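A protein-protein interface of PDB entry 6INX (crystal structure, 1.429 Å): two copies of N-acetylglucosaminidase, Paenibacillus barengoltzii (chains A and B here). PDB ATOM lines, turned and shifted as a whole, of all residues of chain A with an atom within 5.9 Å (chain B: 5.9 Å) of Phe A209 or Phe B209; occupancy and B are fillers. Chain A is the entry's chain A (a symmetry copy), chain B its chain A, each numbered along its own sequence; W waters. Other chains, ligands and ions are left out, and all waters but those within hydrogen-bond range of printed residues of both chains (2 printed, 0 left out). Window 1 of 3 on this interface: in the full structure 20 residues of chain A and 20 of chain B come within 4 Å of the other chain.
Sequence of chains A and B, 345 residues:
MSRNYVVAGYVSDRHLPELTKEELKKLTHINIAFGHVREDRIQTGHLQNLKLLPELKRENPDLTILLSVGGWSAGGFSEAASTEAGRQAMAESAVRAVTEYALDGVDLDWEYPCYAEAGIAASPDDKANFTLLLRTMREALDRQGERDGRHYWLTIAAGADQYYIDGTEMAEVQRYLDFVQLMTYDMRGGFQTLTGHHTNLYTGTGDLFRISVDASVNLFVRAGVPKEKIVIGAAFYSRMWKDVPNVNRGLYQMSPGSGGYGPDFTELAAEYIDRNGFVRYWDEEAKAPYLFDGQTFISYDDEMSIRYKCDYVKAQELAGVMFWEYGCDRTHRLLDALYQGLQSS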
ATOM      1  N   TYR A 163       7.559 -22.201 -21.723  1.00  0.00           N
ATOM      2  CA  TYR A 163       7.048 -23.210 -20.797  1.00  0.00           C
ATOM      3  C   TYR A 163       7.862 -24.494 -20.870  1.00  0.00           C
ATOM      4  O   TYR A 163       8.078 -25.160 -19.848  1.00  0.00           O
ATOM      5  CB  TYR A 163       5.563 -23.501 -21.067  1.00  0.00           C
ATOM      6  CG  TYR A 163       5.290 -24.153 -22.410  1.00  0.00           C
ATOM      7  CD1 TYR A 163       4.974 -23.389 -23.527  1.00  0.00           C
ATOM      8  CD2 TYR A 163       5.364 -25.536 -22.571  1.00  0.00           C
ATOM      9  CE1 TYR A 163       4.738 -23.984 -24.760  1.00  0.00           C
ATOM     10  CE2 TYR A 163       5.138 -26.133 -23.813  1.00  0.00           C
ATOM     11  CZ  TYR A 163       4.828 -25.343 -24.895  1.00  0.00           C
ATOM     12  OH  TYR A 163       4.600 -25.919 -26.123  1.00  0.00           O
ATOM     13  N   ARG A 188       0.693 -20.799 -32.018  1.00  0.00           N
ATOM     14  CA  ARG A 188      -0.536 -20.101 -31.689  1.00  0.00           C
ATOM     15  C   ARG A 188      -1.651 -21.002 -32.183  1.00  0.00           C
ATOM     16  O   ARG A 188      -1.629 -21.435 -33.338  1.00  0.00           O
ATOM     17  CB  ARG A 188      -0.597 -18.763 -32.422  1.00  0.00           C
ATOM     18  CG  ARG A 188       0.536 -17.839 -32.008  1.00  0.00           C
ATOM     19  CD  ARG A 188       0.701 -16.654 -32.964  1.00  0.00           C
ATOM     20  NE  ARG A 188       1.807 -15.824 -32.501  1.00  0.00           N
ATOM     21  CZ  ARG A 188       3.100 -16.127 -32.621  1.00  0.00           C
ATOM     22  NH1 ARG A 188       3.480 -17.259 -33.206  1.00  0.00           N
ATOM     23  NH2 ARG A 188       4.023 -15.314 -32.120  1.00  0.00           N
ATOM     24  N   PHE A 191      -5.127 -22.467 -27.468  1.00  0.00           N
ATOM     25  CA  PHE A 191      -5.160 -21.776 -26.184  1.00  0.00           C
ATOM     26  C   PHE A 191      -5.288 -20.262 -26.302  1.00  0.00           C
ATOM     27  O   PHE A 191      -5.348 -19.582 -25.273  1.00  0.00           O
ATOM     28  CB  PHE A 191      -3.920 -22.121 -25.353  1.00  0.00           C
ATOM     29  CG  PHE A 191      -3.838 -23.575 -24.980  1.00  0.00           C
ATOM     30  CD1 PHE A 191      -4.752 -24.117 -24.101  1.00  0.00           C
ATOM     31  CD2 PHE A 191      -2.874 -24.401 -25.537  1.00  0.00           C
ATOM     32  CE1 PHE A 191      -4.695 -25.463 -23.754  1.00  0.00           C
ATOM     33  CE2 PHE A 191      -2.819 -25.747 -25.194  1.00  0.00           C
ATOM     34  CZ  PHE A 191      -3.732 -26.269 -24.302  1.00  0.00           C
ATOM     35  N   GLN A 192      -5.353 -19.707 -27.513  1.00  0.00           N
ATOM     36  CA  GLN A 192      -5.449 -18.260 -27.646  1.00  0.00           C
ATOM     37  C   GLN A 192      -6.539 -17.866 -28.633  1.00  0.00           C
ATOM     38  O   GLN A 192      -6.761 -18.532 -29.648  1.00  0.00           O
ATOM     39  CB  GLN A 192      -4.090 -17.618 -28.009  1.00  0.00           C
ATOM     40  CG  GLN A 192      -3.570 -17.982 -29.384  1.00  0.00           C
ATOM     41  CD  GLN A 192      -2.218 -17.356 -29.643  1.00  0.00           C
ATOM     42  OE1 GLN A 192      -1.208 -17.775 -29.068  1.00  0.00           O
ATOM     43  NE2 GLN A 192      -2.195 -16.320 -30.492  1.00  0.00           N
ATOM     44  N   LEU A 194      -6.413 -14.719 -29.950  1.00  0.00           N
ATOM     45  CA  LEU A 194      -5.797 -13.745 -30.844  1.00  0.00           C
ATOM     46  C   LEU A 194      -5.236 -14.472 -32.060  1.00  0.00           C
ATOM     47  O   LEU A 194      -4.534 -15.476 -31.914  1.00  0.00           O
ATOM     48  CB  LEU A 194      -4.648 -13.038 -30.125  1.00  0.00           C
ATOM     49  CG  LEU A 194      -4.139 -11.829 -30.905  1.00  0.00           C
ATOM     50  CD1 LEU A 194      -5.155 -10.701 -30.856  1.00  0.00           C
ATOM     51  CD2 LEU A 194      -2.803 -11.362 -30.330  1.00  0.00           C
ATOM     52  N   THR A 203       9.424 -13.660 -35.454  1.00  0.00           N
ATOM     53  CA  THR A 203       8.406 -12.950 -34.690  1.00  0.00           C
ATOM     54  C   THR A 203       8.071 -11.629 -35.372  1.00  0.00           C
ATOM     55  O   THR A 203       8.956 -10.922 -35.854  1.00  0.00           O
ATOM     56  CB  THR A 203       8.909 -12.706 -33.269  1.00  0.00           C
ATOM     57  OG1 THR A 203       9.221 -13.971 -32.669  1.00  0.00           O
ATOM     58  CG2 THR A 203       7.859 -11.984 -32.425  1.00  0.00           C
ATOM     59  N   GLY A 204       6.784 -11.316 -35.441  1.00  0.00           N
ATOM     60  CA  GLY A 204       6.320 -10.112 -36.102  1.00  0.00           C
ATOM     61  C   GLY A 204       5.999  -8.972 -35.152  1.00  0.00           C
ATOM     62  O   GLY A 204       5.555  -9.186 -34.024  1.00  0.00           O
ATOM     63  N   ASP A 207       2.505  -8.330 -32.528  1.00  0.00           N
ATOM     64  CA  ASP A 207       1.933  -9.554 -31.972  1.00  0.00           C
ATOM     65  C   ASP A 207       2.166  -9.576 -30.463  1.00  0.00           C
ATOM     66  O   ASP A 207       3.308  -9.466 -30.015  1.00  0.00           O
ATOM     67  CB  ASP A 207       2.623 -10.762 -32.612  1.00  0.00           C
ATOM     68  CG  ASP A 207       1.893 -12.068 -32.348  1.00  0.00           C
ATOM     69  OD1 ASP A 207       0.965 -12.080 -31.516  1.00  0.00           O
ATOM     70  OD2 ASP A 207       2.267 -13.091 -32.971  1.00  0.00           O
ATOM     71  N   LEU A 208       1.087  -9.725 -29.678  1.00  0.00           N
ATOM     72  CA  LEU A 208       1.251  -9.841 -28.226  1.00  0.00           C
ATOM     73  C   LEU A 208       2.011 -11.104 -27.847  1.00  0.00           C
ATOM     74  O   LEU A 208       2.648 -11.152 -26.787  1.00  0.00           O
ATOM     75  CB  LEU A 208      -0.113  -9.849 -27.524  1.00  0.00           C
ATOM     76  CG  LEU A 208      -0.923  -8.554 -27.593  1.00  0.00           C
ATOM     77  CD1 LEU A 208      -2.278  -8.751 -26.917  1.00  0.00           C
ATOM     78  CD2 LEU A 208      -0.186  -7.381 -26.968  1.00  0.00           C
ATOM     79  N   PHE A 209       1.958 -12.131 -28.689  1.00  0.00           N
ATOM     80  CA  PHE A 209       2.670 -13.381 -28.471  1.00  0.00           C
ATOM     81  C   PHE A 209       3.963 -13.319 -29.271  1.00  0.00           C
ATOM     82  O   PHE A 209       3.955 -12.885 -30.427  1.00  0.00           O
ATOM     83  CB  PHE A 209       1.785 -14.545 -28.913  1.00  0.00           C
ATOM     84  CG  PHE A 209       0.530 -14.672 -28.094  1.00  0.00           C
ATOM     85  CD1 PHE A 209       0.514 -15.471 -26.959  1.00  0.00           C
ATOM     86  CD2 PHE A 209      -0.614 -13.984 -28.435  1.00  0.00           C
ATOM     87  CE1 PHE A 209      -0.633 -15.575 -26.186  1.00  0.00           C
ATOM     88  CE2 PHE A 209      -1.770 -14.083 -27.660  1.00  0.00           C
ATOM     89  CZ  PHE A 209      -1.771 -14.890 -26.542  1.00  0.00           C
ATOM     90  N   ARG A 210       5.082 -13.685 -28.640  1.00  0.00           N
ATOM     91  CA  ARG A 210       6.401 -13.362 -29.180  1.00  0.00           C
ATOM     92  C   ARG A 210       7.177 -14.568 -29.705  1.00  0.00           C
ATOM     93  O   ARG A 210       8.336 -14.412 -30.096  1.00  0.00           O
ATOM     94  CB  ARG A 210       7.234 -12.582 -28.157  1.00  0.00           C
ATOM     95  CG  ARG A 210       6.505 -11.376 -27.541  1.00  0.00           C
ATOM     96  CD  ARG A 210       6.037 -10.359 -28.582  1.00  0.00           C
ATOM     97  NE  ARG A 210       7.151  -9.727 -29.274  1.00  0.00           N
ATOM     98  CZ  ARG A 210       7.057  -9.159 -30.472  1.00  0.00           C
ATOM     99  NH1 ARG A 210       5.897  -9.147 -31.119  1.00  0.00           N
ATOM    100  NH2 ARG A 210       8.140  -8.621 -31.023  1.00  0.00           N
ATOM    101  N   ILE A 211       6.572 -15.751 -29.745  1.00  0.00           N
ATOM    102  CA  ILE A 211       7.280 -16.957 -30.165  1.00  0.00           C
ATOM    103  C   ILE A 211       7.344 -17.048 -31.692  1.00  0.00           C
ATOM    104  O   ILE A 211       6.548 -16.449 -32.420  1.00  0.00           O
ATOM    105  CB  ILE A 211       6.633 -18.205 -29.528  1.00  0.00           C
ATOM    106  CG1 ILE A 211       7.560 -19.434 -29.577  1.00  0.00           C
ATOM    107  CG2 ILE A 211       5.302 -18.506 -30.195  1.00  0.00           C
ATOM    108  CD1 ILE A 211       8.905 -19.261 -28.880  1.00  0.00           C
ATOM    109  N   TYR B 163       5.860  -8.720 -24.657  1.00  0.00           N
ATOM    110  CA  TYR B 163       5.444  -7.869 -25.770  1.00  0.00           C
ATOM    111  C   TYR B 163       5.717  -6.400 -25.478  1.00  0.00           C
ATOM    112  O   TYR B 163       6.079  -5.636 -26.383  1.00  0.00           O
ATOM    113  CB  TYR B 163       3.958  -8.082 -26.099  1.00  0.00           C
ATOM    114  CG  TYR B 163       3.008  -7.638 -25.002  1.00  0.00           C
ATOM    115  CD1 TYR B 163       2.554  -8.533 -24.040  1.00  0.00           C
ATOM    116  CD2 TYR B 163       2.572  -6.317 -24.914  1.00  0.00           C
ATOM    117  CE1 TYR B 163       1.695  -8.124 -23.028  1.00  0.00           C
ATOM    118  CE2 TYR B 163       1.717  -5.903 -23.890  1.00  0.00           C
ATOM    119  CZ  TYR B 163       1.291  -6.818 -22.957  1.00  0.00           C
ATOM    120  OH  TYR B 163       0.447  -6.425 -21.944  1.00  0.00           O
ATOM    121  N   ARG B 188      -3.548 -12.887 -17.642  1.00  0.00           N
ATOM    122  CA  ARG B 188      -4.272 -13.917 -18.365  1.00  0.00           C
ATOM    123  C   ARG B 188      -5.714 -13.450 -18.386  1.00  0.00           C
ATOM    124  O   ARG B 188      -6.268 -13.108 -17.339  1.00  0.00           O
ATOM    125  CB  ARG B 188      -4.177 -15.249 -17.625  1.00  0.00           C
ATOM    126  CG  ARG B 188      -2.741 -15.736 -17.522  1.00  0.00           C
ATOM    127  CD  ARG B 188      -2.581 -16.866 -16.500  1.00  0.00           C
ATOM    128  NE  ARG B 188      -1.181 -17.270 -16.458  1.00  0.00           N
ATOM    129  CZ  ARG B 188      -0.198 -16.580 -15.879  1.00  0.00           C
ATOM    130  NH1 ARG B 188      -0.447 -15.427 -15.267  1.00  0.00           N
ATOM    131  NH2 ARG B 188       1.053 -17.025 -15.942  1.00  0.00           N
ATOM    132  N   PHE B 191      -7.427 -12.866 -24.147  1.00  0.00           N
ATOM    133  CA  PHE B 191      -6.752 -13.449 -25.302  1.00  0.00           C
ATOM    134  C   PHE B 191      -6.427 -14.929 -25.144  1.00  0.00           C
ATOM    135  O   PHE B 191      -5.875 -15.525 -26.074  1.00  0.00           O
ATOM    136  CB  PHE B 191      -5.470 -12.675 -25.625  1.00  0.00           C
ATOM    137  CG  PHE B 191      -5.720 -11.249 -26.032  1.00  0.00           C
ATOM    138  CD1 PHE B 191      -6.356 -10.971 -27.223  1.00  0.00           C
ATOM    139  CD2 PHE B 191      -5.354 -10.197 -25.206  1.00  0.00           C
ATOM    140  CE1 PHE B 191      -6.603  -9.657 -27.609  1.00  0.00           C
ATOM    141  CE2 PHE B 191      -5.604  -8.885 -25.589  1.00  0.00           C
ATOM    142  CZ  PHE B 191      -6.228  -8.624 -26.791  1.00  0.00           C
ATOM    143  N   GLN B 192      -6.764 -15.552 -24.014  1.00  0.00           N
ATOM    144  CA  GLN B 192      -6.438 -16.960 -23.835  1.00  0.00           C
ATOM    145  C   GLN B 192      -7.633 -17.743 -23.308  1.00  0.00           C
ATOM    146  O   GLN B 192      -8.421 -17.248 -22.497  1.00  0.00           O
ATOM    147  CB  GLN B 192      -5.188 -17.159 -22.945  1.00  0.00           C
ATOM    148  CG  GLN B 192      -5.370 -16.737 -21.503  1.00  0.00           C
ATOM    149  CD  GLN B 192      -4.093 -16.917 -20.714  1.00  0.00           C
ATOM    150  OE1 GLN B 192      -3.130 -16.163 -20.892  1.00  0.00           O
ATOM    151  NE2 GLN B 192      -4.064 -17.944 -19.854  1.00  0.00           N
ATOM    152  N   LEU B 194      -7.021 -20.763 -21.843  1.00  0.00           N
ATOM    153  CA  LEU B 194      -6.512 -21.546 -20.722  1.00  0.00           C
ATOM    154  C   LEU B 194      -6.713 -20.759 -19.433  1.00  0.00           C
ATOM    155  O   LEU B 194      -6.366 -19.577 -19.368  1.00  0.00           O
ATOM    156  CB  LEU B 194      -5.017 -21.804 -20.908  1.00  0.00           C
ATOM    157  CG  LEU B 194      -4.483 -22.836 -19.918  1.00  0.00           C
ATOM    158  CD1 LEU B 194      -4.991 -24.223 -20.274  1.00  0.00           C
ATOM    159  CD2 LEU B 194      -2.957 -22.817 -19.915  1.00  0.00           C
ATOM    160  N   THR B 203       5.020 -17.087 -10.719  1.00  0.00           N
ATOM    161  CA  THR B 203       4.648 -18.033 -11.763  1.00  0.00           C
ATOM    162  C   THR B 203       4.520 -19.433 -11.175  1.00  0.00           C
ATOM    163  O   THR B 203       5.333 -19.852 -10.351  1.00  0.00           O
ATOM    164  CB  THR B 203       5.699 -18.014 -12.871  1.00  0.00           C
ATOM    165  OG1 THR B 203       5.795 -16.679 -13.389  1.00  0.00           O
ATOM    166  CG2 THR B 203       5.333 -18.976 -14.001  1.00  0.00           C
ATOM    167  N   GLY B 204       3.473 -20.143 -11.577  1.00  0.00           N
ATOM    168  CA  GLY B 204       3.202 -21.472 -11.063  1.00  0.00           C
ATOM    169  C   GLY B 204       3.643 -22.591 -11.989  1.00  0.00           C
ATOM    170  O   GLY B 204       3.615 -22.458 -13.213  1.00  0.00           O
ATOM    171  N   ASP B 207       1.797 -24.140 -15.690  1.00  0.00           N
ATOM    172  CA  ASP B 207       1.120 -23.128 -16.498  1.00  0.00           C
ATOM    173  C   ASP B 207       1.885 -22.937 -17.805  1.00  0.00           C
ATOM    174  O   ASP B 207       3.081 -22.650 -17.782  1.00  0.00           O
ATOM    175  CB  ASP B 207       1.095 -21.807 -15.723  1.00  0.00           C
ATOM    176  CG  ASP B 207       0.145 -20.787 -16.326  1.00  0.00           C
ATOM    177  OD1 ASP B 207      -0.353 -21.017 -17.446  1.00  0.00           O
ATOM    178  OD2 ASP B 207      -0.090 -19.740 -15.675  1.00  0.00           O
ATOM    179  N   LEU B 208       1.194 -23.088 -18.947  1.00  0.00           N
ATOM    180  CA  LEU B 208       1.847 -22.833 -20.234  1.00  0.00           C
ATOM    181  C   LEU B 208       2.250 -21.373 -20.379  1.00  0.00           C
ATOM    182  O   LEU B 208       3.188 -21.058 -21.121  1.00  0.00           O
ATOM    183  CB  LEU B 208       0.923 -23.215 -21.398  1.00  0.00           C
ATOM    184  CG  LEU B 208       0.603 -24.701 -21.557  1.00  0.00           C
ATOM    185  CD1 LEU B 208      -0.384 -24.902 -22.704  1.00  0.00           C
ATOM    186  CD2 LEU B 208       1.852 -25.537 -21.781  1.00  0.00           C
ATOM    187  N   PHE B 209       1.561 -20.472 -19.687  1.00  0.00           N
ATOM    188  CA  PHE B 209       1.865 -19.050 -19.700  1.00  0.00           C
ATOM    189  C   PHE B 209       2.708 -18.749 -18.470  1.00  0.00           C
ATOM    190  O   PHE B 209       2.403 -19.236 -17.377  1.00  0.00           O
ATOM    191  CB  PHE B 209       0.558 -18.258 -19.699  1.00  0.00           C
ATOM    192  CG  PHE B 209      -0.265 -18.484 -20.937  1.00  0.00           C
ATOM    193  CD1 PHE B 209      -0.105 -17.660 -22.043  1.00  0.00           C
ATOM    194  CD2 PHE B 209      -1.170 -19.520 -21.009  1.00  0.00           C
ATOM    195  CE1 PHE B 209      -0.845 -17.877 -23.197  1.00  0.00           C
ATOM    196  CE2 PHE B 209      -1.915 -19.744 -22.167  1.00  0.00           C
ATOM    197  CZ  PHE B 209      -1.751 -18.910 -23.253  1.00  0.00           C
ATOM    198  N   ARG B 210       3.803 -18.006 -18.654  1.00  0.00           N
ATOM    199  CA  ARG B 210       4.850 -17.927 -17.638  1.00  0.00           C
ATOM    200  C   ARG B 210       4.944 -16.574 -16.937  1.00  0.00           C
ATOM    201  O   ARG B 210       5.855 -16.379 -16.129  1.00  0.00           O
ATOM    202  CB  ARG B 210       6.208 -18.336 -18.219  1.00  0.00           C
ATOM    203  CG  ARG B 210       6.189 -19.668 -18.986  1.00  0.00           C
ATOM    204  CD  ARG B 210       5.713 -20.846 -18.134  1.00  0.00           C
ATOM    205  NE  ARG B 210       6.622 -21.134 -17.035  1.00  0.00           N
ATOM    206  CZ  ARG B 210       6.269 -21.778 -15.927  1.00  0.00           C
ATOM    207  NH1 ARG B 210       5.020 -22.200 -15.765  1.00  0.00           N
ATOM    208  NH2 ARG B 210       7.174 -21.978 -14.975  1.00  0.00           N
ATOM    209  N   ILE B 211       4.027 -15.649 -17.204  1.00  0.00           N
ATOM    210  CA  ILE B 211       4.101 -14.310 -16.626  1.00  0.00           C
ATOM    211  C   ILE B 211       3.553 -14.302 -15.197  1.00  0.00           C
ATOM    212  O   ILE B 211       2.776 -15.168 -14.785  1.00  0.00           O
ATOM    213  CB  ILE B 211       3.382 -13.295 -17.538  1.00  0.00           C
ATOM    214  CG1 ILE B 211       3.780 -11.841 -17.222  1.00  0.00           C
ATOM    215  CG2 ILE B 211       1.878 -13.476 -17.443  1.00  0.00           C
ATOM    216  CD1 ILE B 211       5.268 -11.532 -17.348  1.00  0.00           C
HETATM  217  O   HOH W   1       4.453 -11.314 -24.530  1.00  0.00           O
HETATM  218  O   HOH W   2       5.558 -20.186 -22.537  1.00  0.00           O
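O of Leu A194 is in hydrogen-bond range of NE2 of Gln A192, at 2.9 Å.
OG1 of Thr A203 is in hydrogen-bond range of O of Arg A210 (2.8 Å).
OD1 of Asp A207 lies within hydrogen-bond range of N of Phe A209, at 3.0 Å.
The guanidinium group of Arg B210 sits at hydrogen-bond distance from the backbone carbonyl oxygen of Gly B204 (2.9 Å).
The guanidinium group (NH1) of Arg A210 is in hydrogen-bond range of the backbone carbonyl oxygen (O) of Gly A204.
NE2 of Gln B192 is in hydrogen-bond range of O of Leu B194 (2.9 Å).
Leu B208 touches Tyr A163 (O to CB, 3.4 Å).
Tyr A163 touches Arg B210 (CA to CD, 3.8 Å).
Phe A191 touches Gln B192 (O to CA, 3.2 Å).
Leu B194 touches Phe A191.
CD1 of Leu B208 touches CE2 of Phe A191 (3.6 Å).
Phe B191 touches Gln A192.
CB of Tyr B163 touches O of Leu A208, at 3.4 Å.
CE2 of Phe B191 touches CD1 of Leu A208, at 3.6 Å.
CE1 of Phe A209 touches CE1 of Phe B209, 3.8 Å away.
Tyr B163 touches Arg A210.
Gly A204 touches none of the printed residues of chain B.
Of the printed residues of chain B, Leu A208 touches Tyr B163 and Phe B191.
Phe A209 touches just one residue of chain B: Phe B209.
Ile A211 touches none of the printed residues of chain B.
Of the printed residues of chain A, Tyr B163 touches Leu A208 (3.4 Å) and Arg A210 (3.8 Å).
Of the printed residues of chain A, Leu B194 touches Phe A191.
Of the printed residues of chain A, Phe B209 touches Phe A209.
The nearest residue of chain B that does not touch Phe A209 is Phe B191 (4.2 Å).
The nearest residue of chain A that does not touch Phe B209 is Phe A191 (4.2 Å).
The nearest printed residue of chain A that does not touch Arg B210 is Phe A209 (9.1 Å).
Hydrophobic or aromatic side chains of chain A that line the printed part of chain B: Tyr A163, Phe A191, Leu A194, Leu A208 and Phe A209.
Of the 12 printed residues of chain B, 7 touch a printed residue of chain A.
Printed residues of chain B that touch a printed residue of chain A: Tyr B163, Phe B191, Gln B192, Leu B194, Leu B208, Phe B209 and Arg B210.
Tyr A163 touches Leu B208, and with the chains exchanged Leu A208 touches Tyr B163.
Tyr A163 touches Arg B210, and with the chains exchanged Arg A210 touches Tyr B163.
Phe A191 touches Leu B194, and with the chains exchanged Leu A194 touches Phe B191.
Phe A191 touches Leu B208, and with the chains exchanged Leu A208 touches Phe B191.
Positions printed for both chains: 163, 188, 191, 192, 194, 203, 204, 207, 208, 209, 210 and 211.
Of the 11 pairs that touch across the chains among the printed residues, 11 have their exchanged pair printed and touching as well.
Water W2 bridges the backbone carbonyl oxygen (O) of Leu B208 and the backbone NH (N) of Tyr A163.
Water W1 lies within hydrogen-bond range of the backbone carbonyl oxygen (O) of Leu A208 (2.9 Å) and the backbone NH (N) of Tyr B163 (3.0 Å).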
